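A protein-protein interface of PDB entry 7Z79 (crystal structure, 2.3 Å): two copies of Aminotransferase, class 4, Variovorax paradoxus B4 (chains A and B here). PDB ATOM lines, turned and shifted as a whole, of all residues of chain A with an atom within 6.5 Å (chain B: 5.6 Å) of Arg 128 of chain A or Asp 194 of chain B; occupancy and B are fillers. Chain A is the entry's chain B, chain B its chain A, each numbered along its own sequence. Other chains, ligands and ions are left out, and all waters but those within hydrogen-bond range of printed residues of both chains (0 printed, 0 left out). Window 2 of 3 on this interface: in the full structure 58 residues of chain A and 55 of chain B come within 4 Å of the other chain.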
ATOM      1  N   ARG A 117      36.682 -35.978  16.595  1.00  0.00           N
ATOM      2  CA  ARG A 117      35.243 -35.761  16.497  1.00  0.00           C
ATOM      3  C   ARG A 117      34.628 -36.665  15.425  1.00  0.00           C
ATOM      4  O   ARG A 117      33.483 -37.079  15.552  1.00  0.00           O
ATOM      5  CB  ARG A 117      34.854 -34.284  16.288  1.00  0.00           C
ATOM      6  CG  ARG A 117      33.380 -34.011  16.598  1.00  0.00           C
ATOM      7  CD  ARG A 117      33.097 -32.532  16.291  1.00  0.00           C
ATOM      8  NE  ARG A 117      33.979 -31.751  17.201  1.00  0.00           N
ATOM      9  CZ  ARG A 117      33.657 -31.337  18.425  1.00  0.00           C
ATOM     10  NH1 ARG A 117      32.476 -31.586  18.972  1.00  0.00           N
ATOM     11  NH2 ARG A 117      34.528 -30.670  19.138  1.00  0.00           N
ATOM     12  N   LYS A 120      34.448 -35.565   8.521  1.00  0.00           N
ATOM     13  CA  LYS A 120      33.669 -34.399   8.112  1.00  0.00           C
ATOM     14  C   LYS A 120      33.180 -34.531   6.668  1.00  0.00           C
ATOM     15  O   LYS A 120      33.869 -35.138   5.859  1.00  0.00           O
ATOM     16  CB  LYS A 120      34.573 -33.184   8.273  1.00  0.00           C
ATOM     17  CG  LYS A 120      34.805 -32.814   9.734  1.00  0.00           C
ATOM     18  CD  LYS A 120      35.906 -31.789   9.896  1.00  0.00           C
ATOM     19  CE  LYS A 120      35.744 -30.983  11.171  1.00  0.00           C
ATOM     20  NZ  LYS A 120      34.555 -30.090  11.151  1.00  0.00           N
ATOM     21  N   LYS A 121      32.028 -33.939   6.339  1.00  0.00           N
ATOM     22  CA  LYS A 121      31.522 -33.909   4.960  1.00  0.00           C
ATOM     23  C   LYS A 121      32.437 -33.029   4.110  1.00  0.00           C
ATOM     24  O   LYS A 121      32.588 -33.233   2.925  1.00  0.00           O
ATOM     25  CB  LYS A 121      30.076 -33.428   4.825  1.00  0.00           C
ATOM     26  CG  LYS A 121      29.001 -34.031   5.724  1.00  0.00           C
ATOM     27  CD  LYS A 121      27.662 -34.156   4.953  1.00  0.00           C
ATOM     28  CE  LYS A 121      26.404 -33.980   5.789  1.00  0.00           C
ATOM     29  NZ  LYS A 121      26.268 -35.123   6.733  1.00  0.00           N
ATOM     30  N   GLN A 125      36.345 -26.133  10.269  1.00  0.00           N
ATOM     31  CA  GLN A 125      36.374 -26.250  11.715  1.00  0.00           C
ATOM     32  C   GLN A 125      34.999 -26.602  12.278  1.00  0.00           C
ATOM     33  O   GLN A 125      34.915 -27.018  13.434  1.00  0.00           O
ATOM     34  CB  GLN A 125      36.941 -24.972  12.330  1.00  0.00           C
ATOM     35  CG  GLN A 125      35.935 -23.835  12.380  1.00  0.00           C
ATOM     36  CD  GLN A 125      36.557 -22.636  13.073  1.00  0.00           C
ATOM     37  OE1 GLN A 125      36.203 -22.286  14.213  1.00  0.00           O
ATOM     38  NE2 GLN A 125      37.542 -22.013  12.444  1.00  0.00           N
ATOM     39  N   ASP A 126      33.926 -26.486  11.482  1.00  0.00           N
ATOM     40  CA  ASP A 126      32.598 -26.451  12.068  1.00  0.00           C
ATOM     41  C   ASP A 126      32.256 -27.842  12.607  1.00  0.00           C
ATOM     42  O   ASP A 126      32.211 -28.774  11.843  1.00  0.00           O
ATOM     43  CB  ASP A 126      31.598 -25.928  11.058  1.00  0.00           C
ATOM     44  CG  ASP A 126      30.196 -25.697  11.644  1.00  0.00           C
ATOM     45  OD1 ASP A 126      29.688 -26.547  12.480  1.00  0.00           O
ATOM     46  OD2 ASP A 126      29.595 -24.630  11.270  1.00  0.00           O
ATOM     47  N   PRO A 127      31.960 -28.044  13.909  1.00  0.00           N
ATOM     48  CA  PRO A 127      31.719 -29.401  14.435  1.00  0.00           C
ATOM     49  C   PRO A 127      30.383 -30.032  14.045  1.00  0.00           C
ATOM     50  O   PRO A 127      30.092 -31.195  14.384  1.00  0.00           O
ATOM     51  CB  PRO A 127      31.748 -29.185  15.953  1.00  0.00           C
ATOM     52  CG  PRO A 127      31.231 -27.738  16.090  1.00  0.00           C
ATOM     53  CD  PRO A 127      31.879 -26.986  14.947  1.00  0.00           C
ATOM     54  N   ARG A 128      29.565 -29.303  13.287  1.00  0.00           N
ATOM     55  CA  ARG A 128      28.222 -29.800  12.966  1.00  0.00           C
ATOM     56  C   ARG A 128      28.222 -30.796  11.821  1.00  0.00           C
ATOM     57  O   ARG A 128      27.274 -31.591  11.729  1.00  0.00           O
ATOM     58  CB  ARG A 128      27.274 -28.643  12.617  1.00  0.00           C
ATOM     59  CG  ARG A 128      26.778 -27.954  13.883  1.00  0.00           C
ATOM     60  CD  ARG A 128      25.952 -26.769  13.457  1.00  0.00           C
ATOM     61  NE  ARG A 128      26.845 -25.737  12.989  1.00  0.00           N
ATOM     62  CZ  ARG A 128      26.510 -24.435  12.915  1.00  0.00           C
ATOM     63  NH1 ARG A 128      25.321 -24.045  13.355  1.00  0.00           N
ATOM     64  NH2 ARG A 128      27.395 -23.541  12.524  1.00  0.00           N
ATOM     65  N   PHE A 129      29.257 -30.697  10.970  1.00  0.00           N
ATOM     66  CA  PHE A 129      29.311 -31.387   9.691  1.00  0.00           C
ATOM     67  C   PHE A 129      29.863 -32.836   9.801  1.00  0.00           C
ATOM     68  O   PHE A 129      30.753 -33.105   8.971  1.00  0.00           O
ATOM     69  CB  PHE A 129      30.231 -30.567   8.744  1.00  0.00           C
ATOM     70  CG  PHE A 129      29.796 -29.286   8.053  1.00  0.00           C
ATOM     71  CD1 PHE A 129      30.071 -28.027   8.605  1.00  0.00           C
ATOM     72  CD2 PHE A 129      29.273 -29.304   6.749  1.00  0.00           C
ATOM     73  CE1 PHE A 129      29.768 -26.839   7.929  1.00  0.00           C
ATOM     74  CE2 PHE A 129      28.976 -28.118   6.069  1.00  0.00           C
ATOM     75  CZ  PHE A 129      29.243 -26.880   6.650  1.00  0.00           C
ATOM     76  N   ILE A 130      29.387 -33.704  10.760  1.00  0.00           N
ATOM     77  CA  ILE A 130      30.070 -34.949  11.071  1.00  0.00           C
ATOM     78  C   ILE A 130      29.228 -36.098  10.517  1.00  0.00           C
ATOM     79  O   ILE A 130      28.132 -36.300  10.986  1.00  0.00           O
ATOM     80  CB  ILE A 130      30.411 -35.191  12.582  1.00  0.00           C
ATOM     81  CG1 ILE A 130      31.412 -34.252  13.230  1.00  0.00           C
ATOM     82  CG2 ILE A 130      30.795 -36.625  12.898  1.00  0.00           C
ATOM     83  CD1 ILE A 130      32.842 -34.322  12.705  1.00  0.00           C
ATOM     84  N   ILE A 131      29.766 -36.887   9.571  1.00  0.00           N
ATOM     85  CA  ILE A 131      29.189 -38.152   9.168  1.00  0.00           C
ATOM     86  C   ILE A 131      29.571 -39.178  10.251  1.00  0.00           C
ATOM     87  O   ILE A 131      30.766 -39.439  10.479  1.00  0.00           O
ATOM     88  CB  ILE A 131      29.780 -38.591   7.795  1.00  0.00           C
ATOM     89  CG1 ILE A 131      29.854 -37.474   6.742  1.00  0.00           C
ATOM     90  CG2 ILE A 131      29.095 -39.871   7.268  1.00  0.00           C
ATOM     91  CD1 ILE A 131      30.704 -37.800   5.523  1.00  0.00           C
ATOM     92  N   GLY B 153      22.264 -13.479   5.613  1.00  0.00           N
ATOM     93  CA  GLY B 153      23.197 -13.048   6.598  1.00  0.00           C
ATOM     94  C   GLY B 153      23.279 -13.928   7.841  1.00  0.00           C
ATOM     95  O   GLY B 153      22.317 -14.557   8.276  1.00  0.00           O
ATOM     96  N   LEU B 154      24.489 -13.873   8.400  1.00  0.00           N
ATOM     97  CA  LEU B 154      24.867 -14.679   9.544  1.00  0.00           C
ATOM     98  C   LEU B 154      24.429 -13.987  10.827  1.00  0.00           C
ATOM     99  O   LEU B 154      24.514 -12.758  10.957  1.00  0.00           O
ATOM    100  CB  LEU B 154      26.378 -14.782   9.526  1.00  0.00           C
ATOM    101  CG  LEU B 154      26.981 -15.569   8.377  1.00  0.00           C
ATOM    102  CD1 LEU B 154      28.490 -15.597   8.517  1.00  0.00           C
ATOM    103  CD2 LEU B 154      26.466 -17.005   8.320  1.00  0.00           C
ATOM    104  N   LYS B 155      23.981 -14.812  11.770  1.00  0.00           N
ATOM    105  CA  LYS B 155      23.885 -14.412  13.137  1.00  0.00           C
ATOM    106  C   LYS B 155      25.220 -14.685  13.837  1.00  0.00           C
ATOM    107  O   LYS B 155      25.761 -15.787  13.792  1.00  0.00           O
ATOM    108  CB  LYS B 155      22.752 -15.192  13.815  1.00  0.00           C
ATOM    109  CG  LYS B 155      21.361 -14.939  13.269  1.00  0.00           C
ATOM    110  CD  LYS B 155      20.360 -15.986  13.704  1.00  0.00           C
ATOM    111  CE  LYS B 155      18.952 -15.673  13.202  1.00  0.00           C
ATOM    112  NZ  LYS B 155      18.208 -16.939  12.929  1.00  0.00           N
ATOM    113  N   LEU B 156      25.739 -13.653  14.522  1.00  0.00           N
ATOM    114  CA  LEU B 156      26.968 -13.752  15.276  1.00  0.00           C
ATOM    115  C   LEU B 156      26.647 -13.711  16.767  1.00  0.00           C
ATOM    116  O   LEU B 156      25.700 -13.020  17.188  1.00  0.00           O
ATOM    117  CB  LEU B 156      27.789 -12.548  14.888  1.00  0.00           C
ATOM    118  CG  LEU B 156      28.827 -12.756  13.802  1.00  0.00           C
ATOM    119  CD1 LEU B 156      28.409 -13.723  12.736  1.00  0.00           C
ATOM    120  CD2 LEU B 156      29.256 -11.444  13.177  1.00  0.00           C
ATOM    121  N   LEU B 185      33.110 -21.120  18.559  1.00  0.00           N
ATOM    122  CA  LEU B 185      32.024 -21.435  17.675  1.00  0.00           C
ATOM    123  C   LEU B 185      30.995 -22.259  18.431  1.00  0.00           C
ATOM    124  O   LEU B 185      29.793 -21.983  18.288  1.00  0.00           O
ATOM    125  CB  LEU B 185      32.539 -22.108  16.401  1.00  0.00           C
ATOM    126  CG  LEU B 185      31.461 -22.628  15.448  1.00  0.00           C
ATOM    127  CD1 LEU B 185      30.557 -21.456  14.941  1.00  0.00           C
ATOM    128  CD2 LEU B 185      32.063 -23.441  14.283  1.00  0.00           C
ATOM    129  N   ALA B 188      28.881 -20.046  20.437  1.00  0.00           N
ATOM    130  CA  ALA B 188      28.003 -19.294  19.583  1.00  0.00           C
ATOM    131  C   ALA B 188      26.854 -20.169  19.057  1.00  0.00           C
ATOM    132  O   ALA B 188      25.708 -19.723  19.053  1.00  0.00           O
ATOM    133  CB  ALA B 188      28.766 -18.662  18.475  1.00  0.00           C
ATOM    134  N   ILE B 189      27.137 -21.422  18.665  1.00  0.00           N
ATOM    135  CA  ILE B 189      26.096 -22.271  18.131  1.00  0.00           C
ATOM    136  C   ILE B 189      25.027 -22.446  19.210  1.00  0.00           C
ATOM    137  O   ILE B 189      23.840 -22.276  18.924  1.00  0.00           O
ATOM    138  CB  ILE B 189      26.616 -23.607  17.579  1.00  0.00           C
ATOM    139  CG1 ILE B 189      27.456 -23.424  16.314  1.00  0.00           C
ATOM    140  CG2 ILE B 189      25.500 -24.645  17.395  1.00  0.00           C
ATOM    141  CD1 ILE B 189      28.400 -24.579  16.053  1.00  0.00           C
ATOM    142  N   GLY B 192      22.372 -19.947  19.484  1.00  0.00           N
ATOM    143  CA  GLY B 192      21.476 -19.777  18.346  1.00  0.00           C
ATOM    144  C   GLY B 192      22.164 -18.971  17.250  1.00  0.00           C
ATOM    145  O   GLY B 192      21.499 -18.527  16.357  1.00  0.00           O
ATOM    146  N   ALA B 193      23.488 -18.814  17.292  1.00  0.00           N
ATOM    147  CA  ALA B 193      24.176 -18.061  16.248  1.00  0.00           C
ATOM    148  C   ALA B 193      24.849 -18.990  15.226  1.00  0.00           C
ATOM    149  O   ALA B 193      24.968 -20.176  15.446  1.00  0.00           O
ATOM    150  CB  ALA B 193      25.156 -17.105  16.863  1.00  0.00           C
ATOM    151  N   ASP B 194      25.311 -18.431  14.094  1.00  0.00           N
ATOM    152  CA  ASP B 194      25.927 -19.199  13.039  1.00  0.00           C
ATOM    153  C   ASP B 194      27.453 -19.238  13.161  1.00  0.00           C
ATOM    154  O   ASP B 194      28.125 -20.147  12.637  1.00  0.00           O
ATOM    155  CB  ASP B 194      25.551 -18.603  11.696  1.00  0.00           C
ATOM    156  CG  ASP B 194      24.047 -18.559  11.506  1.00  0.00           C
ATOM    157  OD1 ASP B 194      23.420 -19.634  11.701  1.00  0.00           O
ATOM    158  OD2 ASP B 194      23.530 -17.452  11.135  1.00  0.00           O
ATOM    159  N   GLU B 195      28.015 -18.201  13.798  1.00  0.00           N
ATOM    160  CA  GLU B 195      29.431 -17.906  13.832  1.00  0.00           C
ATOM    161  C   GLU B 195      29.710 -17.183  15.140  1.00  0.00           C
ATOM    162  O   GLU B 195      28.825 -16.523  15.637  1.00  0.00           O
ATOM    163  CB  GLU B 195      29.703 -17.180  12.539  1.00  0.00           C
ATOM    164  CG  GLU B 195      31.143 -16.820  12.266  1.00  0.00           C
ATOM    165  CD  GLU B 195      31.925 -17.825  11.460  1.00  0.00           C
ATOM    166  OE1 GLU B 195      31.253 -18.849  11.145  1.00  0.00           O
ATOM    167  OE2 GLU B 195      33.184 -17.572  11.192  1.00  0.00           O
ATOM    168  N   ALA B 196      30.889 -17.414  15.750  1.00  0.00           N
ATOM    169  CA  ALA B 196      31.324 -16.653  16.922  1.00  0.00           C
ATOM    170  C   ALA B 196      32.029 -15.404  16.469  1.00  0.00           C
ATOM    171  O   ALA B 196      32.861 -15.465  15.551  1.00  0.00           O
ATOM    172  CB  ALA B 196      32.235 -17.475  17.801  1.00  0.00           C
ATOM    173  N   ASN B 209      35.287 -16.693  14.281  1.00  0.00           N
ATOM    174  CA  ASN B 209      36.068 -17.915  14.492  1.00  0.00           C
ATOM    175  C   ASN B 209      36.674 -18.430  13.178  1.00  0.00           C
ATOM    176  O   ASN B 209      37.647 -19.147  13.211  1.00  0.00           O
ATOM    177  CB  ASN B 209      35.274 -18.983  15.236  1.00  0.00           C
ATOM    178  CG  ASN B 209      34.033 -19.322  14.397  1.00  0.00           C
ATOM    179  OD1 ASN B 209      33.065 -18.565  14.381  1.00  0.00           O
ATOM    180  ND2 ASN B 209      34.050 -20.413  13.639  1.00  0.00           N
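NH2 of Arg 128 of chain A is in hydrogen-bond range of O of Asp 194 of chain B (3.5 Å).
The side-chain amide nitrogen (ND2) of Asn 209 of chain B sits at hydrogen-bond distance from the side-chain amide oxygen (OE1) of Gln 125 of chain A, 2.9 Å away.
O of Lys 155 of chain B is in hydrogen-bond range of N of Asp 194 of chain B, at 2.7 Å.
The side-chain carboxylate (OE2) of Glu 195 of chain B lies close to the side-chain amide oxygen (OD1) of Asn 209 of chain B, at 3.3 Å.
N of Ala 196 of chain B lies within hydrogen-bond range of OD1 of Asn 209 of chain B, 2.8 Å away.
NZ of Lys 120 of chain A lies within hydrogen-bond range of O of Asp 126 of chain A (2.8 Å).
OD2 of Asp 126 of chain A lies within salt-bridge range of NH2 of Arg 128 of chain A (2.8 Å).
Among the printed residues, pairs that only touch across the chains: Asp 126 of chain A with Leu 185 of chain B, Pro 127 of chain A with Leu 185 of chain B and Arg 128 of chain A with Ile 189 of chain B.
Arg 117 of chain A touches none of the printed residues of chain B.
Of the printed residues of chain B, Asp 126 of chain A touches Leu 185.
Of the printed residues of chain B, Pro 127 of chain A touches Leu 185 (3.6 Å).
Printed residues of chain B within 4 Å of Arg 128 of chain A: Ile 189 (3.6 Å) and Asp 194 (3.5 Å).
Asp 194 of chain B touches just one residue of chain A: Arg 128 (3.5 Å).
Glu 195 of chain B touches none of the printed residues of chain A.
Printed residues of chain A within 4 Å of Asn 209 of chain B: Gln 125 (2.9 Å).
Of the 10 printed residues of chain A, 4 touch a printed residue of chain B.
Along chain B the printed residues that touch a printed residue of chain A span positions 185 to 209.
Among the printed residues, 5 pairs touch across the chains.
No position is printed for both chains.
Of the 5 pairs that touch across the chains among the printed residues, none has its exchanged pair printed and touching as well.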
